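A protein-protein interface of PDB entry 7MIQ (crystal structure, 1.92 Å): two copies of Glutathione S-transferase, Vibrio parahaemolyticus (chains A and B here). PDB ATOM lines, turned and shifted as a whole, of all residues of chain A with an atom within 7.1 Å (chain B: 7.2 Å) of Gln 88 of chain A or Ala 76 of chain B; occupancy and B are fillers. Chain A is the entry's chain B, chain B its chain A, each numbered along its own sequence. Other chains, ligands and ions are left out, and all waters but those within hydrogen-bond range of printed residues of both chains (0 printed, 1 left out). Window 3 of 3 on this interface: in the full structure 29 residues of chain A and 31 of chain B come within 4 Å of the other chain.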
ATOM      1  N   GLY A  85       8.267   7.214   9.042  1.00  0.00           N
ATOM      2  CA  GLY A  85       9.396   7.236   8.100  1.00  0.00           C
ATOM      3  C   GLY A  85       9.444   8.577   7.396  1.00  0.00           C
ATOM      4  O   GLY A  85       8.439   9.093   6.915  1.00  0.00           O
ATOM      5  N   ALA A  86      10.648   9.153   7.332  1.00  0.00           N
ATOM      6  CA  ALA A  86      10.787  10.524   6.846  1.00  0.00           C
ATOM      7  C   ALA A  86      10.898  10.609   5.327  1.00  0.00           C
ATOM      8  O   ALA A  86      10.592  11.660   4.750  1.00  0.00           O
ATOM      9  CB  ALA A  86      12.003  11.191   7.495  1.00  0.00           C
ATOM     10  N   ASN A  87      11.338   9.540   4.663  1.00  0.00           N
ATOM     11  CA  ASN A  87      11.430   9.529   3.209  1.00  0.00           C
ATOM     12  C   ASN A  87      10.935   8.180   2.698  1.00  0.00           C
ATOM     13  O   ASN A  87      10.522   7.315   3.476  1.00  0.00           O
ATOM     14  CB  ASN A  87      12.859   9.838   2.732  1.00  0.00           C
ATOM     15  CG  ASN A  87      13.902   8.905   3.332  1.00  0.00           C
ATOM     16  OD1 ASN A  87      13.706   7.693   3.406  1.00  0.00           O
ATOM     17  ND2 ASN A  87      15.025   9.475   3.756  1.00  0.00           N
ATOM     18  N   GLN A  88      10.990   8.008   1.374  1.00  0.00           N
ATOM     19  CA  GLN A  88      10.463   6.798   0.740  1.00  0.00           C
ATOM     20  C   GLN A  88      11.123   5.541   1.296  1.00  0.00           C
ATOM     21  O   GLN A  88      10.440   4.574   1.657  1.00  0.00           O
ATOM     22  CB  GLN A  88      10.660   6.883  -0.776  1.00  0.00           C
ATOM     23  CG  GLN A  88      10.303   5.611  -1.542  1.00  0.00           C
ATOM     24  CD  GLN A  88      10.656   5.718  -3.020  1.00  0.00           C
ATOM     25  OE1 GLN A  88      11.118   6.761  -3.481  1.00  0.00           O
ATOM     26  NE2 GLN A  88      10.442   4.637  -3.765  1.00  0.00           N
ATOM     27  N   LEU A  89      12.458   5.529   1.365  1.00  0.00           N
ATOM     28  CA  LEU A  89      13.148   4.349   1.877  1.00  0.00           C
ATOM     29  C   LEU A  89      12.798   4.094   3.337  1.00  0.00           C
ATOM     30  O   LEU A  89      12.508   2.954   3.721  1.00  0.00           O
ATOM     31  CB  LEU A  89      14.662   4.498   1.707  1.00  0.00           C
ATOM     32  CG  LEU A  89      15.494   3.330   2.244  1.00  0.00           C
ATOM     33  CD1 LEU A  89      15.030   2.022   1.626  1.00  0.00           C
ATOM     34  CD2 LEU A  89      16.977   3.549   1.975  1.00  0.00           C
ATOM     35  N   GLU A  90      12.824   5.140   4.169  1.00  0.00           N
ATOM     36  CA  GLU A  90      12.494   4.961   5.581  1.00  0.00           C
ATOM     37  C   GLU A  90      11.074   4.435   5.759  1.00  0.00           C
ATOM     38  O   GLU A  90      10.817   3.623   6.657  1.00  0.00           O
ATOM     39  CB  GLU A  90      12.669   6.276   6.344  1.00  0.00           C
ATOM     40  CG  GLU A  90      14.110   6.719   6.490  1.00  0.00           C
ATOM     41  CD  GLU A  90      14.279   7.871   7.463  1.00  0.00           C
ATOM     42  OE1 GLU A  90      13.295   8.236   8.147  1.00  0.00           O
ATOM     43  OE2 GLU A  90      15.404   8.403   7.549  1.00  0.00           O
ATOM     44  N   ARG A  91      10.138   4.891   4.925  1.00  0.00           N
ATOM     45  CA  ARG A  91       8.762   4.416   5.045  1.00  0.00           C
ATOM     46  C   ARG A  91       8.677   2.918   4.786  1.00  0.00           C
ATOM     47  O   ARG A  91       7.925   2.208   5.464  1.00  0.00           O
ATOM     48  CB  ARG A  91       7.847   5.191   4.094  1.00  0.00           C
ATOM     49  CG  ARG A  91       7.496   6.587   4.608  1.00  0.00           C
ATOM     50  CD  ARG A  91       6.414   7.269   3.778  1.00  0.00           C
ATOM     51  NE  ARG A  91       6.916   7.782   2.507  1.00  0.00           N
ATOM     52  CZ  ARG A  91       7.572   8.926   2.366  1.00  0.00           C
ATOM     53  NH1 ARG A  91       7.862   9.690   3.407  1.00  0.00           N
ATOM     54  NH2 ARG A  91       7.945   9.314   1.150  1.00  0.00           N
ATOM     55  N   ALA A  92       9.454   2.416   3.822  1.00  0.00           N
ATOM     56  CA  ALA A  92       9.470   0.981   3.548  1.00  0.00           C
ATOM     57  C   ALA A  92      10.221   0.214   4.632  1.00  0.00           C
ATOM     58  O   ALA A  92       9.841  -0.910   4.981  1.00  0.00           O
ATOM     59  CB  ALA A  92      10.092   0.716   2.177  1.00  0.00           C
ATOM     60  N   GLN A  93      11.296   0.796   5.166  1.00  0.00           N
ATOM     61  CA  GLN A  93      12.026   0.133   6.242  1.00  0.00           C
ATOM     62  C   GLN A  93      11.198   0.091   7.518  1.00  0.00           C
ATOM     63  O   GLN A  93      11.204  -0.915   8.240  1.00  0.00           O
ATOM     64  CB  GLN A  93      13.361   0.838   6.479  1.00  0.00           C
ATOM     65  CG  GLN A  93      14.359   0.626   5.352  1.00  0.00           C
ATOM     66  CD  GLN A  93      15.561   1.547   5.446  1.00  0.00           C
ATOM     67  OE1 GLN A  93      15.453   2.690   5.896  1.00  0.00           O
ATOM     68  NE2 GLN A  93      16.720   1.051   5.015  1.00  0.00           N
ATOM     69  N   VAL A  94      10.466   1.168   7.806  1.00  0.00           N
ATOM     70  CA  VAL A  94       9.560   1.163   8.951  1.00  0.00           C
ATOM     71  C   VAL A  94       8.527   0.051   8.802  1.00  0.00           C
ATOM     72  O   VAL A  94       8.294  -0.727   9.734  1.00  0.00           O
ATOM     73  CB  VAL A  94       8.900   2.543   9.120  1.00  0.00           C
ATOM     74  CG1 VAL A  94       7.627   2.438   9.952  1.00  0.00           C
ATOM     75  CG2 VAL A  94       9.880   3.507   9.775  1.00  0.00           C
ATOM     76  N   MET B   1      16.074  -1.868 -10.032  1.00  0.00           N
ATOM     77  CA  MET B   1      16.045  -2.743  -8.870  1.00  0.00           C
ATOM     78  C   MET B   1      15.789  -4.191  -9.280  1.00  0.00           C
ATOM     79  O   MET B   1      15.493  -4.468 -10.440  1.00  0.00           O
ATOM     80  CB  MET B   1      14.985  -2.270  -7.875  1.00  0.00           C
ATOM     81  CG  MET B   1      13.729  -1.721  -8.506  1.00  0.00           C
ATOM     82  SD  MET B   1      12.746  -0.764  -7.332  1.00  0.00           S
ATOM     83  CE  MET B   1      11.670   0.112  -8.457  1.00  0.00           C
ATOM     84  N   ILE B  22      -0.066  -1.339 -10.532  1.00  0.00           N
ATOM     85  CA  ILE B  22       0.464   0.016 -10.658  1.00  0.00           C
ATOM     86  C   ILE B  22       1.250   0.221 -11.944  1.00  0.00           C
ATOM     87  O   ILE B  22       1.720   1.339 -12.199  1.00  0.00           O
ATOM     88  CB  ILE B  22       1.338   0.384  -9.442  1.00  0.00           C
ATOM     89  CG1 ILE B  22       2.596  -0.489  -9.390  1.00  0.00           C
ATOM     90  CG2 ILE B  22       0.530   0.254  -8.155  1.00  0.00           C
ATOM     91  CD1 ILE B  22       3.507  -0.157  -8.219  1.00  0.00           C
ATOM     92  N   VAL B  26       9.973  -4.668 -12.793  1.00  0.00           N
ATOM     93  CA  VAL B  26      11.186  -4.888 -12.009  1.00  0.00           C
ATOM     94  C   VAL B  26      11.814  -6.206 -12.445  1.00  0.00           C
ATOM     95  O   VAL B  26      11.109  -7.202 -12.634  1.00  0.00           O
ATOM     96  CB  VAL B  26      10.887  -4.913 -10.493  1.00  0.00           C
ATOM     97  CG1 VAL B  26      12.141  -5.256  -9.701  1.00  0.00           C
ATOM     98  CG2 VAL B  26      10.313  -3.581 -10.033  1.00  0.00           C
ATOM     99  N   LEU B  55      13.288  -7.365  -2.144  1.00  0.00           N
ATOM    100  CA  LEU B  55      13.538  -6.305  -3.114  1.00  0.00           C
ATOM    101  C   LEU B  55      14.924  -5.723  -2.880  1.00  0.00           C
ATOM    102  O   LEU B  55      15.279  -5.394  -1.744  1.00  0.00           O
ATOM    103  CB  LEU B  55      12.486  -5.201  -3.004  1.00  0.00           C
ATOM    104  CG  LEU B  55      12.660  -4.056  -4.002  1.00  0.00           C
ATOM    105  CD1 LEU B  55      12.346  -4.537  -5.414  1.00  0.00           C
ATOM    106  CD2 LEU B  55      11.786  -2.877  -3.616  1.00  0.00           C
ATOM    107  N   LEU B  57      17.410  -2.654  -4.063  1.00  0.00           N
ATOM    108  CA  LEU B  57      17.470  -1.367  -4.737  1.00  0.00           C
ATOM    109  C   LEU B  57      18.776  -1.230  -5.518  1.00  0.00           C
ATOM    110  O   LEU B  57      19.720  -2.006  -5.347  1.00  0.00           O
ATOM    111  CB  LEU B  57      17.340  -0.229  -3.724  1.00  0.00           C
ATOM    112  CG  LEU B  57      16.146  -0.306  -2.777  1.00  0.00           C
ATOM    113  CD1 LEU B  57      16.046   0.953  -1.927  1.00  0.00           C
ATOM    114  CD2 LEU B  57      14.863  -0.544  -3.561  1.00  0.00           C
ATOM    115  N   ILE B  63      14.906  -4.815   0.997  1.00  0.00           N
ATOM    116  CA  ILE B  63      13.644  -4.670   1.713  1.00  0.00           C
ATOM    117  C   ILE B  63      12.921  -6.008   1.639  1.00  0.00           C
ATOM    118  O   ILE B  63      12.721  -6.543   0.544  1.00  0.00           O
ATOM    119  CB  ILE B  63      12.771  -3.553   1.105  1.00  0.00           C
ATOM    120  CG1 ILE B  63      13.506  -2.209   1.147  1.00  0.00           C
ATOM    121  CG2 ILE B  63      11.426  -3.462   1.822  1.00  0.00           C
ATOM    122  CD1 ILE B  63      12.870  -1.131   0.280  1.00  0.00           C
ATOM    123  N   ALA B  68       5.844  -4.267   2.816  1.00  0.00           N
ATOM    124  CA  ALA B  68       6.872  -3.228   2.797  1.00  0.00           C
ATOM    125  C   ALA B  68       7.442  -3.041   1.396  1.00  0.00           C
ATOM    126  O   ALA B  68       7.741  -1.911   0.982  1.00  0.00           O
ATOM    127  CB  ALA B  68       7.981  -3.575   3.791  1.00  0.00           C
ATOM    128  N   CYS B  70       5.720  -3.597  -1.355  1.00  0.00           N
ATOM    129  CA  CYS B  70       4.666  -2.898  -2.088  1.00  0.00           C
ATOM    130  C   CYS B  70       4.643  -1.412  -1.754  1.00  0.00           C
ATOM    131  O   CYS B  70       4.405  -0.576  -2.635  1.00  0.00           O
ATOM    132  CB  CYS B  70       3.305  -3.527  -1.789  1.00  0.00           C
ATOM    133  SG  CYS B  70       3.087  -5.203  -2.446  1.00  0.00           S
ATOM    134  N   ARG B  71       4.871  -1.058  -0.485  1.00  0.00           N
ATOM    135  CA  ARG B  71       4.871   0.355  -0.118  1.00  0.00           C
ATOM    136  C   ARG B  71       5.980   1.110  -0.842  1.00  0.00           C
ATOM    137  O   ARG B  71       5.768   2.230  -1.322  1.00  0.00           O
ATOM    138  CB  ARG B  71       5.003   0.520   1.397  1.00  0.00           C
ATOM    139  CG  ARG B  71       4.891   1.977   1.850  1.00  0.00           C
ATOM    140  CD  ARG B  71       4.898   2.150   3.369  1.00  0.00           C
ATOM    141  NE  ARG B  71       3.808   1.434   4.023  1.00  0.00           N
ATOM    142  CZ  ARG B  71       2.539   1.826   4.022  1.00  0.00           C
ATOM    143  NH1 ARG B  71       2.152   2.917   3.381  1.00  0.00           N
ATOM    144  NH2 ARG B  71       1.637   1.101   4.676  1.00  0.00           N
ATOM    145  N   TYR B  72       7.169   0.510  -0.944  1.00  0.00           N
ATOM    146  CA  TYR B  72       8.251   1.157  -1.683  1.00  0.00           C
ATOM    147  C   TYR B  72       7.912   1.264  -3.165  1.00  0.00           C
ATOM    148  O   TYR B  72       8.095   2.323  -3.782  1.00  0.00           O
ATOM    149  CB  TYR B  72       9.565   0.395  -1.490  1.00  0.00           C
ATOM    150  CG  TYR B  72      10.753   1.125  -2.081  1.00  0.00           C
ATOM    151  CD1 TYR B  72      11.096   0.973  -3.425  1.00  0.00           C
ATOM    152  CD2 TYR B  72      11.516   1.987  -1.304  1.00  0.00           C
ATOM    153  CE1 TYR B  72      12.174   1.655  -3.973  1.00  0.00           C
ATOM    154  CE2 TYR B  72      12.596   2.667  -1.841  1.00  0.00           C
ATOM    155  CZ  TYR B  72      12.918   2.499  -3.174  1.00  0.00           C
ATOM    156  OH  TYR B  72      13.987   3.181  -3.708  1.00  0.00           O
ATOM    157  N   LEU B  73       7.421   0.171  -3.757  1.00  0.00           N
ATOM    158  CA  LEU B  73       7.095   0.175  -5.181  1.00  0.00           C
ATOM    159  C   LEU B  73       5.986   1.161  -5.506  1.00  0.00           C
ATOM    160  O   LEU B  73       5.964   1.722  -6.608  1.00  0.00           O
ATOM    161  CB  LEU B  73       6.690  -1.227  -5.631  1.00  0.00           C
ATOM    162  CG  LEU B  73       7.769  -2.308  -5.560  1.00  0.00           C
ATOM    163  CD1 LEU B  73       7.154  -3.687  -5.816  1.00  0.00           C
ATOM    164  CD2 LEU B  73       8.887  -2.015  -6.543  1.00  0.00           C
ATOM    165  N   ASP B  74       5.050   1.370  -4.575  1.00  0.00           N
ATOM    166  CA  ASP B  74       3.984   2.344  -4.799  1.00  0.00           C
ATOM    167  C   ASP B  74       4.558   3.736  -5.036  1.00  0.00           C
ATOM    168  O   ASP B  74       4.066   4.484  -5.888  1.00  0.00           O
ATOM    169  CB  ASP B  74       3.024   2.347  -3.608  1.00  0.00           C
ATOM    170  CG  ASP B  74       1.757   3.151  -3.874  1.00  0.00           C
ATOM    171  OD1 ASP B  74       1.202   3.046  -4.986  1.00  0.00           O
ATOM    172  OD2 ASP B  74       1.300   3.870  -2.962  1.00  0.00           O
ATOM    173  N   GLU B  75       5.611   4.096  -4.303  1.00  0.00           N
ATOM    174  CA  GLU B  75       6.253   5.386  -4.516  1.00  0.00           C
ATOM    175  C   GLU B  75       7.251   5.356  -5.663  1.00  0.00           C
ATOM    176  O   GLU B  75       7.533   6.406  -6.251  1.00  0.00           O
ATOM    177  CB  GLU B  75       6.949   5.845  -3.235  1.00  0.00           C
ATOM    178  CG  GLU B  75       6.001   6.048  -2.070  1.00  0.00           C
ATOM    179  CD  GLU B  75       6.684   6.648  -0.859  1.00  0.00           C
ATOM    180  OE1 GLU B  75       7.419   7.644  -1.022  1.00  0.00           O
ATOM    181  OE2 GLU B  75       6.492   6.118   0.253  1.00  0.00           O
ATOM    182  N   ALA B  76       7.785   4.178  -5.995  1.00  0.00           N
ATOM    183  CA  ALA B  76       8.753   4.083  -7.081  1.00  0.00           C
ATOM    184  C   ALA B  76       8.093   4.237  -8.444  1.00  0.00           C
ATOM    185  O   ALA B  76       8.701   4.795  -9.363  1.00  0.00           O
ATOM    186  CB  ALA B  76       9.502   2.753  -7.005  1.00  0.00           C
ATOM    187  N   PHE B  77       6.859   3.761  -8.598  1.00  0.00           N
ATOM    188  CA  PHE B  77       6.131   3.844  -9.865  1.00  0.00           C
ATOM    189  C   PHE B  77       4.879   4.683  -9.644  1.00  0.00           C
ATOM    190  O   PHE B  77       3.859   4.172  -9.170  1.00  0.00           O
ATOM    191  CB  PHE B  77       5.793   2.450 -10.392  1.00  0.00           C
ATOM    192  CG  PHE B  77       6.999   1.596 -10.623  1.00  0.00           C
ATOM    193  CD1 PHE B  77       7.771   1.761 -11.761  1.00  0.00           C
ATOM    194  CD2 PHE B  77       7.377   0.644  -9.692  1.00  0.00           C
ATOM    195  CE1 PHE B  77       8.895   0.987 -11.973  1.00  0.00           C
ATOM    196  CE2 PHE B  77       8.499  -0.139  -9.898  1.00  0.00           C
ATOM    197  CZ  PHE B  77       9.259   0.034 -11.041  1.00  0.00           C
ATOM    198  N   GLU B  78       4.963   5.967  -9.991  1.00  0.00           N
ATOM    199  CA  GLU B  78       3.834   6.875  -9.827  1.00  0.00           C
ATOM    200  C   GLU B  78       2.596   6.324 -10.523  1.00  0.00           C
ATOM    201  O   GLU B  78       2.660   5.871 -11.671  1.00  0.00           O
ATOM    202  CB  GLU B  78       4.185   8.256 -10.383  1.00  0.00           C
ATOM    203  CG  GLU B  78       3.063   9.274 -10.263  1.00  0.00           C
ATOM    204  CD  GLU B  78       3.496  10.670 -10.665  1.00  0.00           C
ATOM    205  OE1 GLU B  78       4.578  10.807 -11.275  1.00  0.00           O
ATOM    206  OE2 GLU B  78       2.756  11.631 -10.365  1.00  0.00           O
ATOM    207  N   ASN B  79       1.469   6.355  -9.816  1.00  0.00           N
ATOM    208  CA  ASN B  79       0.222   5.790 -10.305  1.00  0.00           C
ATOM    209  C   ASN B  79      -0.922   6.471  -9.572  1.00  0.00           C
ATOM    210  O   ASN B  79      -0.722   7.106  -8.534  1.00  0.00           O
ATOM    211  CB  ASN B  79       0.173   4.274 -10.090  1.00  0.00           C
ATOM    212  CG  ASN B  79       0.064   3.906  -8.622  1.00  0.00           C
ATOM    213  OD1 ASN B  79      -1.036   3.770  -8.087  1.00  0.00           O
ATOM    214  ND2 ASN B  79       1.205   3.761  -7.959  1.00  0.00           N
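NE2 of Gln 88 of chain A sits at hydrogen-bond distance from O of Tyr 72 of chain B (3.3 Å). The side-chain carboxylate (OE1) of Glu 75 of chain B is in salt-bridge range of the guanidinium group (NH2) of Arg 91 of chain A, at 2.8 Å. N of Ala 76 of chain B lies close to NE2 of Gln 88 of chain A, 3.5 Å away.
O of Leu 55 of chain B lies within hydrogen-bond range of N of Ile 63 of chain B, 2.8 Å away. N of Leu 89 of chain A sits at hydrogen-bond distance from OD1 of Asn 87 of chain A (3.2 Å).
Among the printed residues, merely in contact across the chains: Gln 88 of chain A with Glu 75 of chain B (3.3 Å), Leu 89 of chain A with Leu 57 of chain B (3.8 Å), Arg 91 of chain A with Arg 71 of chain B (3.7 Å), Ala 92 of chain A with Ile 63 of chain B (3.8 Å), Ala 92 of chain A with Ala 68 of chain B (3.5 Å) and Ala 92 of chain A with Tyr 72 of chain B (3.7 Å).
Of the printed residues of chain B, Gln 88 of chain A touches Tyr 72 (3.3 Å), Glu 75 (3.3 Å) and Ala 76 (3.5 Å). Glu 90 of chain A touches none of the printed residues of chain B. Of the printed residues of chain A, Leu 57 of chain B touches Leu 89. Printed residues of chain A within 4 Å of Ala 68 of chain B: Ala 92 (3.5 Å). Asp 74 of chain B touches none of the printed residues of chain A. Of chain A, only Gln 88 comes within 4 Å of Ala 76 of chain B. The nearest residue of chain B that does not touch Gln 88 of chain A is Leu 73 of chain B (5.4 Å). The nearest printed residue of chain B that does not touch Ala 92 of chain A is Arg 71 of chain B (4.6 Å).
Of the 10 printed residues of chain A, 4 touch a printed residue of chain B. Printed residues of chain A that touch a printed residue of chain B: Gln 88, Leu 89, Arg 91 and Ala 92. Hydrophobic or aromatic side chains of chain A that line the printed part of chain B: Leu 89 and Ala 92. Of the 17 printed residues of chain B, 7 touch a printed residue of chain A. Among the printed residues, 9 pairs touch across the chains.
No position is printed for both chains. Of the 9 pairs that touch across the chains among the printed residues, none has its exchanged pair printed and touching as well.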
